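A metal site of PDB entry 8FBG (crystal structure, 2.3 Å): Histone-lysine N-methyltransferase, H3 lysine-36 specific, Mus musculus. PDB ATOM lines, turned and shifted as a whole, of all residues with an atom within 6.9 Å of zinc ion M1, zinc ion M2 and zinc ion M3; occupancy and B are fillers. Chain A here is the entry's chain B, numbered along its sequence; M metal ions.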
ATOM      1  N   PRO A  43      24.194 -19.167   8.902  1.00  0.00           N
ATOM      2  CA  PRO A  43      24.550 -20.441   9.579  1.00  0.00           C
ATOM      3  C   PRO A  43      25.743 -21.117   8.915  1.00  0.00           C
ATOM      4  O   PRO A  43      26.092 -20.795   7.764  1.00  0.00           O
ATOM      5  CB  PRO A  43      23.260 -21.259   9.462  1.00  0.00           C
ATOM      6  CG  PRO A  43      22.560 -20.720   8.267  1.00  0.00           C
ATOM      7  CD  PRO A  43      22.851 -19.246   8.302  1.00  0.00           C
ATOM      8  N   ARG A  44      26.411 -22.012   9.637  1.00  0.00           N
ATOM      9  CA  ARG A  44      27.589 -22.627   9.050  1.00  0.00           C
ATOM     10  C   ARG A  44      27.363 -24.132   8.905  1.00  0.00           C
ATOM     11  O   ARG A  44      27.118 -24.842   9.876  1.00  0.00           O
ATOM     12  CB  ARG A  44      28.836 -22.273   9.885  1.00  0.00           C
ATOM     13  CG  ARG A  44      30.154 -22.457   9.168  1.00  0.00           C
ATOM     14  CD  ARG A  44      30.878 -23.682   9.696  1.00  0.00           C
ATOM     15  NE  ARG A  44      31.202 -23.575  11.117  1.00  0.00           N
ATOM     16  CZ  ARG A  44      32.347 -23.083  11.586  1.00  0.00           C
ATOM     17  N   CYS A  45      27.437 -24.591   7.649  1.00  0.00           N
ATOM     18  CA  CYS A  45      27.259 -25.991   7.275  1.00  0.00           C
ATOM     19  C   CYS A  45      28.471 -26.808   7.700  1.00  0.00           C
ATOM     20  O   CYS A  45      29.531 -26.248   7.971  1.00  0.00           O
ATOM     21  CB  CYS A  45      26.987 -26.128   5.778  1.00  0.00           C
ATOM     22  SG  CYS A  45      28.452 -25.876   4.730  1.00  0.00           S
ATOM     23  N   ASN A  46      28.323 -28.137   7.731  1.00  0.00           N
ATOM     24  CA  ASN A  46      29.430 -28.983   8.113  1.00  0.00           C
ATOM     25  C   ASN A  46      29.920 -29.810   6.915  1.00  0.00           C
ATOM     26  O   ASN A  46      30.531 -30.852   7.104  1.00  0.00           O
ATOM     27  CB  ASN A  46      29.067 -29.866   9.301  1.00  0.00           C
ATOM     28  CG  ASN A  46      30.257 -30.151  10.194  1.00  0.00           C
ATOM     29  OD1 ASN A  46      30.894 -29.227  10.728  1.00  0.00           O
ATOM     30  ND2 ASN A  46      30.590 -31.421  10.379  1.00  0.00           N
ATOM     31  N   CYS A  47      29.717 -29.295   5.685  1.00  0.00           N
ATOM     32  CA  CYS A  47      30.159 -29.955   4.471  1.00  0.00           C
ATOM     33  C   CYS A  47      31.675 -30.002   4.362  1.00  0.00           C
ATOM     34  O   CYS A  47      32.358 -29.159   4.954  1.00  0.00           O
ATOM     35  CB  CYS A  47      29.539 -29.286   3.250  1.00  0.00           C
ATOM     36  SG  CYS A  47      27.761 -29.552   3.135  1.00  0.00           S
ATOM     37  N   LYS A  48      32.186 -31.047   3.702  1.00  0.00           N
ATOM     38  CA  LYS A  48      33.639 -31.233   3.597  1.00  0.00           C
ATOM     39  C   LYS A  48      34.104 -31.088   2.155  1.00  0.00           C
ATOM     40  O   LYS A  48      33.344 -31.316   1.224  1.00  0.00           O
ATOM     41  CB  LYS A  48      34.104 -32.602   4.182  1.00  0.00           C
ATOM     42  CG  LYS A  48      33.154 -33.210   5.198  1.00  0.00           C
ATOM     43  CD  LYS A  48      33.893 -33.740   6.426  1.00  0.00           C
ATOM     44  CE  LYS A  48      33.829 -32.792   7.598  1.00  0.00           C
ATOM     45  NZ  LYS A  48      32.486 -32.744   8.223  1.00  0.00           N
ATOM     46  N   ASP A  51      33.638 -34.138   0.123  1.00  0.00           N
ATOM     47  CA  ASP A  51      32.298 -34.573  -0.341  1.00  0.00           C
ATOM     48  C   ASP A  51      32.238 -34.546  -1.904  1.00  0.00           C
ATOM     49  O   ASP A  51      32.878 -33.698  -2.517  1.00  0.00           O
ATOM     50  CB  ASP A  51      31.182 -33.687   0.254  1.00  0.00           C
ATOM     51  CG  ASP A  51      31.100 -33.663   1.769  1.00  0.00           C
ATOM     52  OD1 ASP A  51      31.687 -34.542   2.412  1.00  0.00           O
ATOM     53  OD2 ASP A  51      30.445 -32.765   2.310  1.00  0.00           O
ATOM     54  N   PRO A  54      30.281 -30.791  -2.904  1.00  0.00           N
ATOM     55  CA  PRO A  54      30.104 -30.117  -1.606  1.00  0.00           C
ATOM     56  C   PRO A  54      29.146 -28.936  -1.694  1.00  0.00           C
ATOM     57  O   PRO A  54      29.319 -28.081  -2.558  1.00  0.00           O
ATOM     58  CB  PRO A  54      31.535 -29.687  -1.224  1.00  0.00           C
ATOM     59  CG  PRO A  54      32.460 -30.388  -2.188  1.00  0.00           C
ATOM     60  CD  PRO A  54      31.664 -30.632  -3.424  1.00  0.00           C
ATOM     61  N   CYS A  55      28.088 -28.940  -0.830  1.00  0.00           N
ATOM     62  CA  CYS A  55      27.019 -27.919  -0.742  1.00  0.00           C
ATOM     63  C   CYS A  55      26.150 -27.875  -2.028  1.00  0.00           C
ATOM     64  O   CYS A  55      25.407 -26.910  -2.213  1.00  0.00           O
ATOM     65  CB  CYS A  55      27.588 -26.531  -0.419  1.00  0.00           C
ATOM     66  SG  CYS A  55      28.867 -26.529   0.875  1.00  0.00           S
ATOM     67  N   GLY A  56      26.252 -28.910  -2.874  1.00  0.00           N
ATOM     68  CA  GLY A  56      25.559 -29.045  -4.155  1.00  0.00           C
ATOM     69  C   GLY A  56      24.075 -29.324  -4.038  1.00  0.00           C
ATOM     70  O   GLY A  56      23.560 -29.426  -2.923  1.00  0.00           O
ATOM     71  N   SER A  59      22.644 -32.938  -1.688  1.00  0.00           N
ATOM     72  CA  SER A  59      23.582 -32.901  -0.559  1.00  0.00           C
ATOM     73  C   SER A  59      22.913 -32.536   0.789  1.00  0.00           C
ATOM     74  O   SER A  59      21.791 -32.002   0.848  1.00  0.00           O
ATOM     75  CB  SER A  59      24.741 -31.935  -0.819  1.00  0.00           C
ATOM     76  OG  SER A  59      24.510 -30.622  -0.315  1.00  0.00           O
ATOM     77  N   GLU A  60      23.675 -32.770   1.867  1.00  0.00           N
ATOM     78  CA  GLU A  60      23.282 -32.525   3.243  1.00  0.00           C
ATOM     79  C   GLU A  60      23.969 -31.248   3.764  1.00  0.00           C
ATOM     80  O   GLU A  60      24.827 -31.286   4.643  1.00  0.00           O
ATOM     81  CB  GLU A  60      23.592 -33.772   4.095  1.00  0.00           C
ATOM     82  CG  GLU A  60      23.120 -35.094   3.472  1.00  0.00           C
ATOM     83  CD  GLU A  60      21.625 -35.377   3.450  1.00  0.00           C
ATOM     84  OE1 GLU A  60      21.219 -36.216   2.624  1.00  0.00           O
ATOM     85  OE2 GLU A  60      20.879 -34.770   4.251  1.00  0.00           O
ATOM     86  N   CYS A  61      23.568 -30.100   3.181  1.00  0.00           N
ATOM     87  CA  CYS A  61      24.066 -28.760   3.505  1.00  0.00           C
ATOM     88  C   CYS A  61      22.964 -28.017   4.222  1.00  0.00           C
ATOM     89  O   CYS A  61      21.926 -27.777   3.615  1.00  0.00           O
ATOM     90  CB  CYS A  61      24.474 -28.054   2.216  1.00  0.00           C
ATOM     91  SG  CYS A  61      25.225 -26.431   2.481  1.00  0.00           S
ATOM     92  N   ILE A  62      23.166 -27.633   5.498  1.00  0.00           N
ATOM     93  CA  ILE A  62      22.137 -26.921   6.279  1.00  0.00           C
ATOM     94  C   ILE A  62      21.746 -25.611   5.539  1.00  0.00           C
ATOM     95  O   ILE A  62      20.556 -25.342   5.380  1.00  0.00           O
ATOM     96  CB  ILE A  62      22.536 -26.670   7.791  1.00  0.00           C
ATOM     97  CG1 ILE A  62      21.302 -26.365   8.683  1.00  0.00           C
ATOM     98  CG2 ILE A  62      23.644 -25.638   7.987  1.00  0.00           C
ATOM     99  N   ASN A  63      22.751 -24.882   5.001  1.00  0.00           N
ATOM    100  CA  ASN A  63      22.520 -23.652   4.272  1.00  0.00           C
ATOM    101  C   ASN A  63      21.638 -23.910   3.015  1.00  0.00           C
ATOM    102  O   ASN A  63      20.652 -23.212   2.835  1.00  0.00           O
ATOM    103  CB  ASN A  63      23.848 -23.014   3.917  1.00  0.00           C
ATOM    104  CG  ASN A  63      24.639 -22.588   5.090  1.00  0.00           C
ATOM    105  OD1 ASN A  63      25.150 -23.416   5.848  1.00  0.00           O
ATOM    106  ND2 ASN A  63      24.787 -21.297   5.273  1.00  0.00           N
ATOM    107  N   ARG A  64      21.956 -24.919   2.203  1.00  0.00           N
ATOM    108  CA  ARG A  64      21.127 -25.203   1.023  1.00  0.00           C
ATOM    109  C   ARG A  64      19.721 -25.645   1.434  1.00  0.00           C
ATOM    110  O   ARG A  64      18.756 -25.180   0.829  1.00  0.00           O
ATOM    111  CB  ARG A  64      21.768 -26.226   0.085  1.00  0.00           C
ATOM    112  CG  ARG A  64      21.000 -26.356  -1.215  1.00  0.00           C
ATOM    113  CD  ARG A  64      21.756 -27.184  -2.213  1.00  0.00           C
ATOM    114  NE  ARG A  64      22.761 -26.422  -2.974  1.00  0.00           N
ATOM    115  CZ  ARG A  64      22.501 -25.774  -4.104  1.00  0.00           C
ATOM    116  NH1 ARG A  64      21.261 -25.720  -4.582  1.00  0.00           N
ATOM    117  NH2 ARG A  64      23.468 -25.143  -4.748  1.00  0.00           N
ATOM    118  N   GLU A  69      22.632 -19.118   1.057  1.00  0.00           N
ATOM    119  CA  GLU A  69      23.873 -19.363   0.337  1.00  0.00           C
ATOM    120  C   GLU A  69      24.901 -19.627   1.462  1.00  0.00           C
ATOM    121  O   GLU A  69      24.702 -19.193   2.611  1.00  0.00           O
ATOM    122  CB  GLU A  69      24.307 -18.073  -0.385  1.00  0.00           C
ATOM    123  CG  GLU A  69      24.122 -18.069  -1.880  1.00  0.00           C
ATOM    124  CD  GLU A  69      24.986 -17.057  -2.618  1.00  0.00           C
ATOM    125  OE1 GLU A  69      25.830 -16.381  -1.989  1.00  0.00           O
ATOM    126  OE2 GLU A  69      24.828 -16.949  -3.842  1.00  0.00           O
ATOM    127  N   CYS A  70      26.009 -20.301   1.144  1.00  0.00           N
ATOM    128  CA  CYS A  70      27.065 -20.453   2.130  1.00  0.00           C
ATOM    129  C   CYS A  70      27.793 -19.131   2.370  1.00  0.00           C
ATOM    130  O   CYS A  70      27.659 -18.212   1.575  1.00  0.00           O
ATOM    131  CB  CYS A  70      28.040 -21.534   1.688  1.00  0.00           C
ATOM    132  SG  CYS A  70      27.406 -23.199   1.891  1.00  0.00           S
ATOM    133  N   HIS A  71      28.576 -19.047   3.455  1.00  0.00           N
ATOM    134  CA  HIS A  71      29.399 -17.884   3.776  1.00  0.00           C
ATOM    135  C   HIS A  71      30.432 -17.745   2.619  1.00  0.00           C
ATOM    136  O   HIS A  71      31.012 -18.759   2.207  1.00  0.00           O
ATOM    137  CB  HIS A  71      30.111 -18.095   5.108  1.00  0.00           C
ATOM    138  CG  HIS A  71      30.621 -16.850   5.766  1.00  0.00           C
ATOM    139  ND1 HIS A  71      31.616 -16.079   5.180  1.00  0.00           N
ATOM    140  CD2 HIS A  71      30.331 -16.330   6.986  1.00  0.00           C
ATOM    141  CE1 HIS A  71      31.852 -15.090   6.022  1.00  0.00           C
ATOM    142  NE2 HIS A  71      31.116 -15.202   7.130  1.00  0.00           N
ATOM    143  N   VAL A  74      33.965 -18.393   4.699  1.00  0.00           N
ATOM    144  CA  VAL A  74      34.073 -19.261   5.875  1.00  0.00           C
ATOM    145  C   VAL A  74      33.465 -20.678   5.671  1.00  0.00           C
ATOM    146  O   VAL A  74      33.503 -21.472   6.632  1.00  0.00           O
ATOM    147  CB  VAL A  74      33.460 -18.582   7.115  1.00  0.00           C
ATOM    148  N   CYS A  75      32.958 -21.036   4.468  1.00  0.00           N
ATOM    149  CA  CYS A  75      32.392 -22.373   4.245  1.00  0.00           C
ATOM    150  C   CYS A  75      33.470 -23.495   4.428  1.00  0.00           C
ATOM    151  O   CYS A  75      34.559 -23.380   3.831  1.00  0.00           O
ATOM    152  CB  CYS A  75      31.714 -22.482   2.885  1.00  0.00           C
ATOM    153  SG  CYS A  75      30.936 -24.095   2.588  1.00  0.00           S
ATOM    154  N   PRO A  76      33.218 -24.564   5.231  1.00  0.00           N
ATOM    155  CA  PRO A  76      34.265 -25.594   5.437  1.00  0.00           C
ATOM    156  C   PRO A  76      34.588 -26.397   4.185  1.00  0.00           C
ATOM    157  O   PRO A  76      35.656 -27.010   4.159  1.00  0.00           O
ATOM    158  CB  PRO A  76      33.693 -26.490   6.529  1.00  0.00           C
ATOM    159  CG  PRO A  76      32.589 -25.712   7.144  1.00  0.00           C
ATOM    160  CD  PRO A  76      32.021 -24.877   6.031  1.00  0.00           C
ATOM    161  N   ALA A  77      33.663 -26.384   3.165  1.00  0.00           N
ATOM    162  CA  ALA A  77      33.858 -27.067   1.868  1.00  0.00           C
ATOM    163  C   ALA A  77      35.008 -26.416   1.047  1.00  0.00           C
ATOM    164  O   ALA A  77      35.602 -27.077   0.178  1.00  0.00           O
ATOM    165  CB  ALA A  77      32.577 -27.077   1.084  1.00  0.00           C
ATOM    166  N   GLY A  78      35.310 -25.149   1.341  1.00  0.00           N
ATOM    167  CA  GLY A  78      36.355 -24.371   0.676  1.00  0.00           C
ATOM    168  C   GLY A  78      35.919 -23.829  -0.672  1.00  0.00           C
ATOM    169  O   GLY A  78      34.732 -23.580  -0.890  1.00  0.00           O
ATOM    170  N   ARG A  80      35.600 -25.361  -3.331  1.00  0.00           N
ATOM    171  CA  ARG A  80      34.729 -26.388  -3.919  1.00  0.00           C
ATOM    172  C   ARG A  80      33.212 -26.165  -3.618  1.00  0.00           C
ATOM    173  O   ARG A  80      32.377 -26.826  -4.233  1.00  0.00           O
ATOM    174  CB  ARG A  80      35.158 -27.785  -3.447  1.00  0.00           C
ATOM    175  CG  ARG A  80      36.602 -28.126  -3.762  1.00  0.00           C
ATOM    176  CD  ARG A  80      36.746 -29.318  -4.672  1.00  0.00           C
ATOM    177  NE  ARG A  80      36.361 -30.560  -4.002  1.00  0.00           N
ATOM    178  CZ  ARG A  80      35.323 -31.316  -4.339  1.00  0.00           C
ATOM    179  NH1 ARG A  80      34.560 -30.976  -5.383  1.00  0.00           N
ATOM    180  NH2 ARG A  80      35.030 -32.404  -3.663  1.00  0.00           N
ATOM    181  N   CYS A  81      32.874 -25.252  -2.674  1.00  0.00           N
ATOM    182  CA  CYS A  81      31.486 -24.998  -2.324  1.00  0.00           C
ATOM    183  C   CYS A  81      30.595 -24.716  -3.561  1.00  0.00           C
ATOM    184  O   CYS A  81      30.874 -23.808  -4.358  1.00  0.00           O
ATOM    185  CB  CYS A  81      31.375 -23.868  -1.306  1.00  0.00           C
ATOM    186  SG  CYS A  81      29.663 -23.330  -1.009  1.00  0.00           S
ATOM    187  N   GLN A  82      29.476 -25.467  -3.685  1.00  0.00           N
ATOM    188  CA  GLN A  82      28.529 -25.307  -4.806  1.00  0.00           C
ATOM    189  C   GLN A  82      27.234 -24.598  -4.399  1.00  0.00           C
ATOM    190  O   GLN A  82      26.223 -24.758  -5.076  1.00  0.00           O
ATOM    191  CB  GLN A  82      28.202 -26.676  -5.416  1.00  0.00           C
ATOM    192  CG  GLN A  82      29.340 -27.330  -6.167  1.00  0.00           C
ATOM    193  CD  GLN A  82      29.018 -28.745  -6.550  1.00  0.00           C
ATOM    194  OE1 GLN A  82      27.851 -29.141  -6.690  1.00  0.00           O
ATOM    195  NE2 GLN A  82      30.061 -29.541  -6.737  1.00  0.00           N
ATOM    196  N   ASN A  83      27.273 -23.823  -3.308  1.00  0.00           N
ATOM    197  CA  ASN A  83      26.134 -23.049  -2.784  1.00  0.00           C
ATOM    198  C   ASN A  83      26.490 -21.515  -2.688  1.00  0.00           C
ATOM    199  O   ASN A  83      26.413 -20.895  -1.631  1.00  0.00           O
ATOM    200  CB  ASN A  83      25.663 -23.638  -1.431  1.00  0.00           C
ATOM    201  CG  ASN A  83      24.375 -23.059  -0.884  1.00  0.00           C
ATOM    202  OD1 ASN A  83      23.518 -22.586  -1.602  1.00  0.00           O
ATOM    203  ND2 ASN A  83      24.214 -23.082   0.435  1.00  0.00           N
ATOM    204  N   GLN A  84      26.885 -20.934  -3.824  1.00  0.00           N
ATOM    205  CA  GLN A  84      27.211 -19.507  -3.964  1.00  0.00           C
ATOM    206  C   GLN A  84      26.672 -19.012  -5.339  1.00  0.00           C
ATOM    207  O   GLN A  84      27.248 -18.115  -5.948  1.00  0.00           O
ATOM    208  CB  GLN A  84      28.743 -19.299  -3.808  1.00  0.00           C
ATOM    209  CG  GLN A  84      29.216 -19.105  -2.354  1.00  0.00           C
ATOM    210  CD  GLN A  84      30.578 -19.707  -2.080  1.00  0.00           C
ATOM    211  OE1 GLN A  84      31.463 -19.753  -2.933  1.00  0.00           O
ATOM    212  NE2 GLN A  84      30.785 -20.194  -0.863  1.00  0.00           N
HETATM  213 ZN    ZN M   1      28.664 -23.747   3.880  1.00  0.00          ZN
HETATM  214 ZN    ZN M   2      27.426 -26.959   2.897  1.00  0.00          ZN
HETATM  215 ZN    ZN M   3      29.376 -24.344   0.868  1.00  0.00          ZN
HETATM  216 CA    CA M   4      28.811 -21.792   5.330  1.00  0.00          CA
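SG of Cys 45 binds zinc ion M1 (2.3 Å).
Zinc ion M1 is bound by SG of Cys 70, at 2.4 Å.
SG of Cys 75 binds zinc ion M1 (2.6 Å).
The backbone NH (N) of Asn 83 lies close to the side-chain sulfur (SG) of Cys 81, at 3.4 Å.
The side-chain sulfur of Cys 81 lies close to the side-chain amide nitrogen of Gln 84 (3.3 Å).
O of Cys 55 lies within hydrogen-bond range of NE of Arg 64 (2.8 Å).
SG of Cys 61 lies close to N of Arg 64, 3.6 Å away.
OD1 of Asn 63 sits at hydrogen-bond distance from N of Cys 45 (3.1 Å).
The side-chain sulfur of Cys 75 sits close to the backbone NH of Ala 77, at 3.6 Å.
The backbone NH (N) of Cys 70 is in hydrogen-bond range of the backbone carbonyl oxygen (O) of Asn 83, at 2.9 Å.
SG of Cys 47 sits close to O of Glu 60 (3.7 Å).
Five residues have an atom within 4 Å of zinc ion M2: Cys 45, Cys 47, Cys 55, Cys 61 and Cys 70.
The nearest printed residue that does not touch zinc ion M2 is Cys 75 (4.5 Å).
SG of Cys 61 binds zinc ion M2.
The side-chain sulfur (SG) of Cys 45 binds zinc ion M2, 2.4 Å away.
Zinc ion M2 is bound by SG of Cys 55.
The side-chain sulfur (SG) of Cys 47 binds zinc ion M2, 2.6 Å away.
Within 4 Å of zinc ion M3: Cys 55, Cys 70, Cys 75 and Cys 81.
The side-chain sulfur (SG) of Cys 81 is bound to zinc ion M3, 2.2 Å away.
SG of Cys 55 is bound to zinc ion M3 (2.2 Å).
SG of Cys 75 is bound to zinc ion M3, 2.3 Å away.
SG of Cys 70 binds zinc ion M3 (2.5 Å).
Three residues have an atom within 4 Å of zinc ion M1: Cys 45, Cys 70 and Cys 75.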
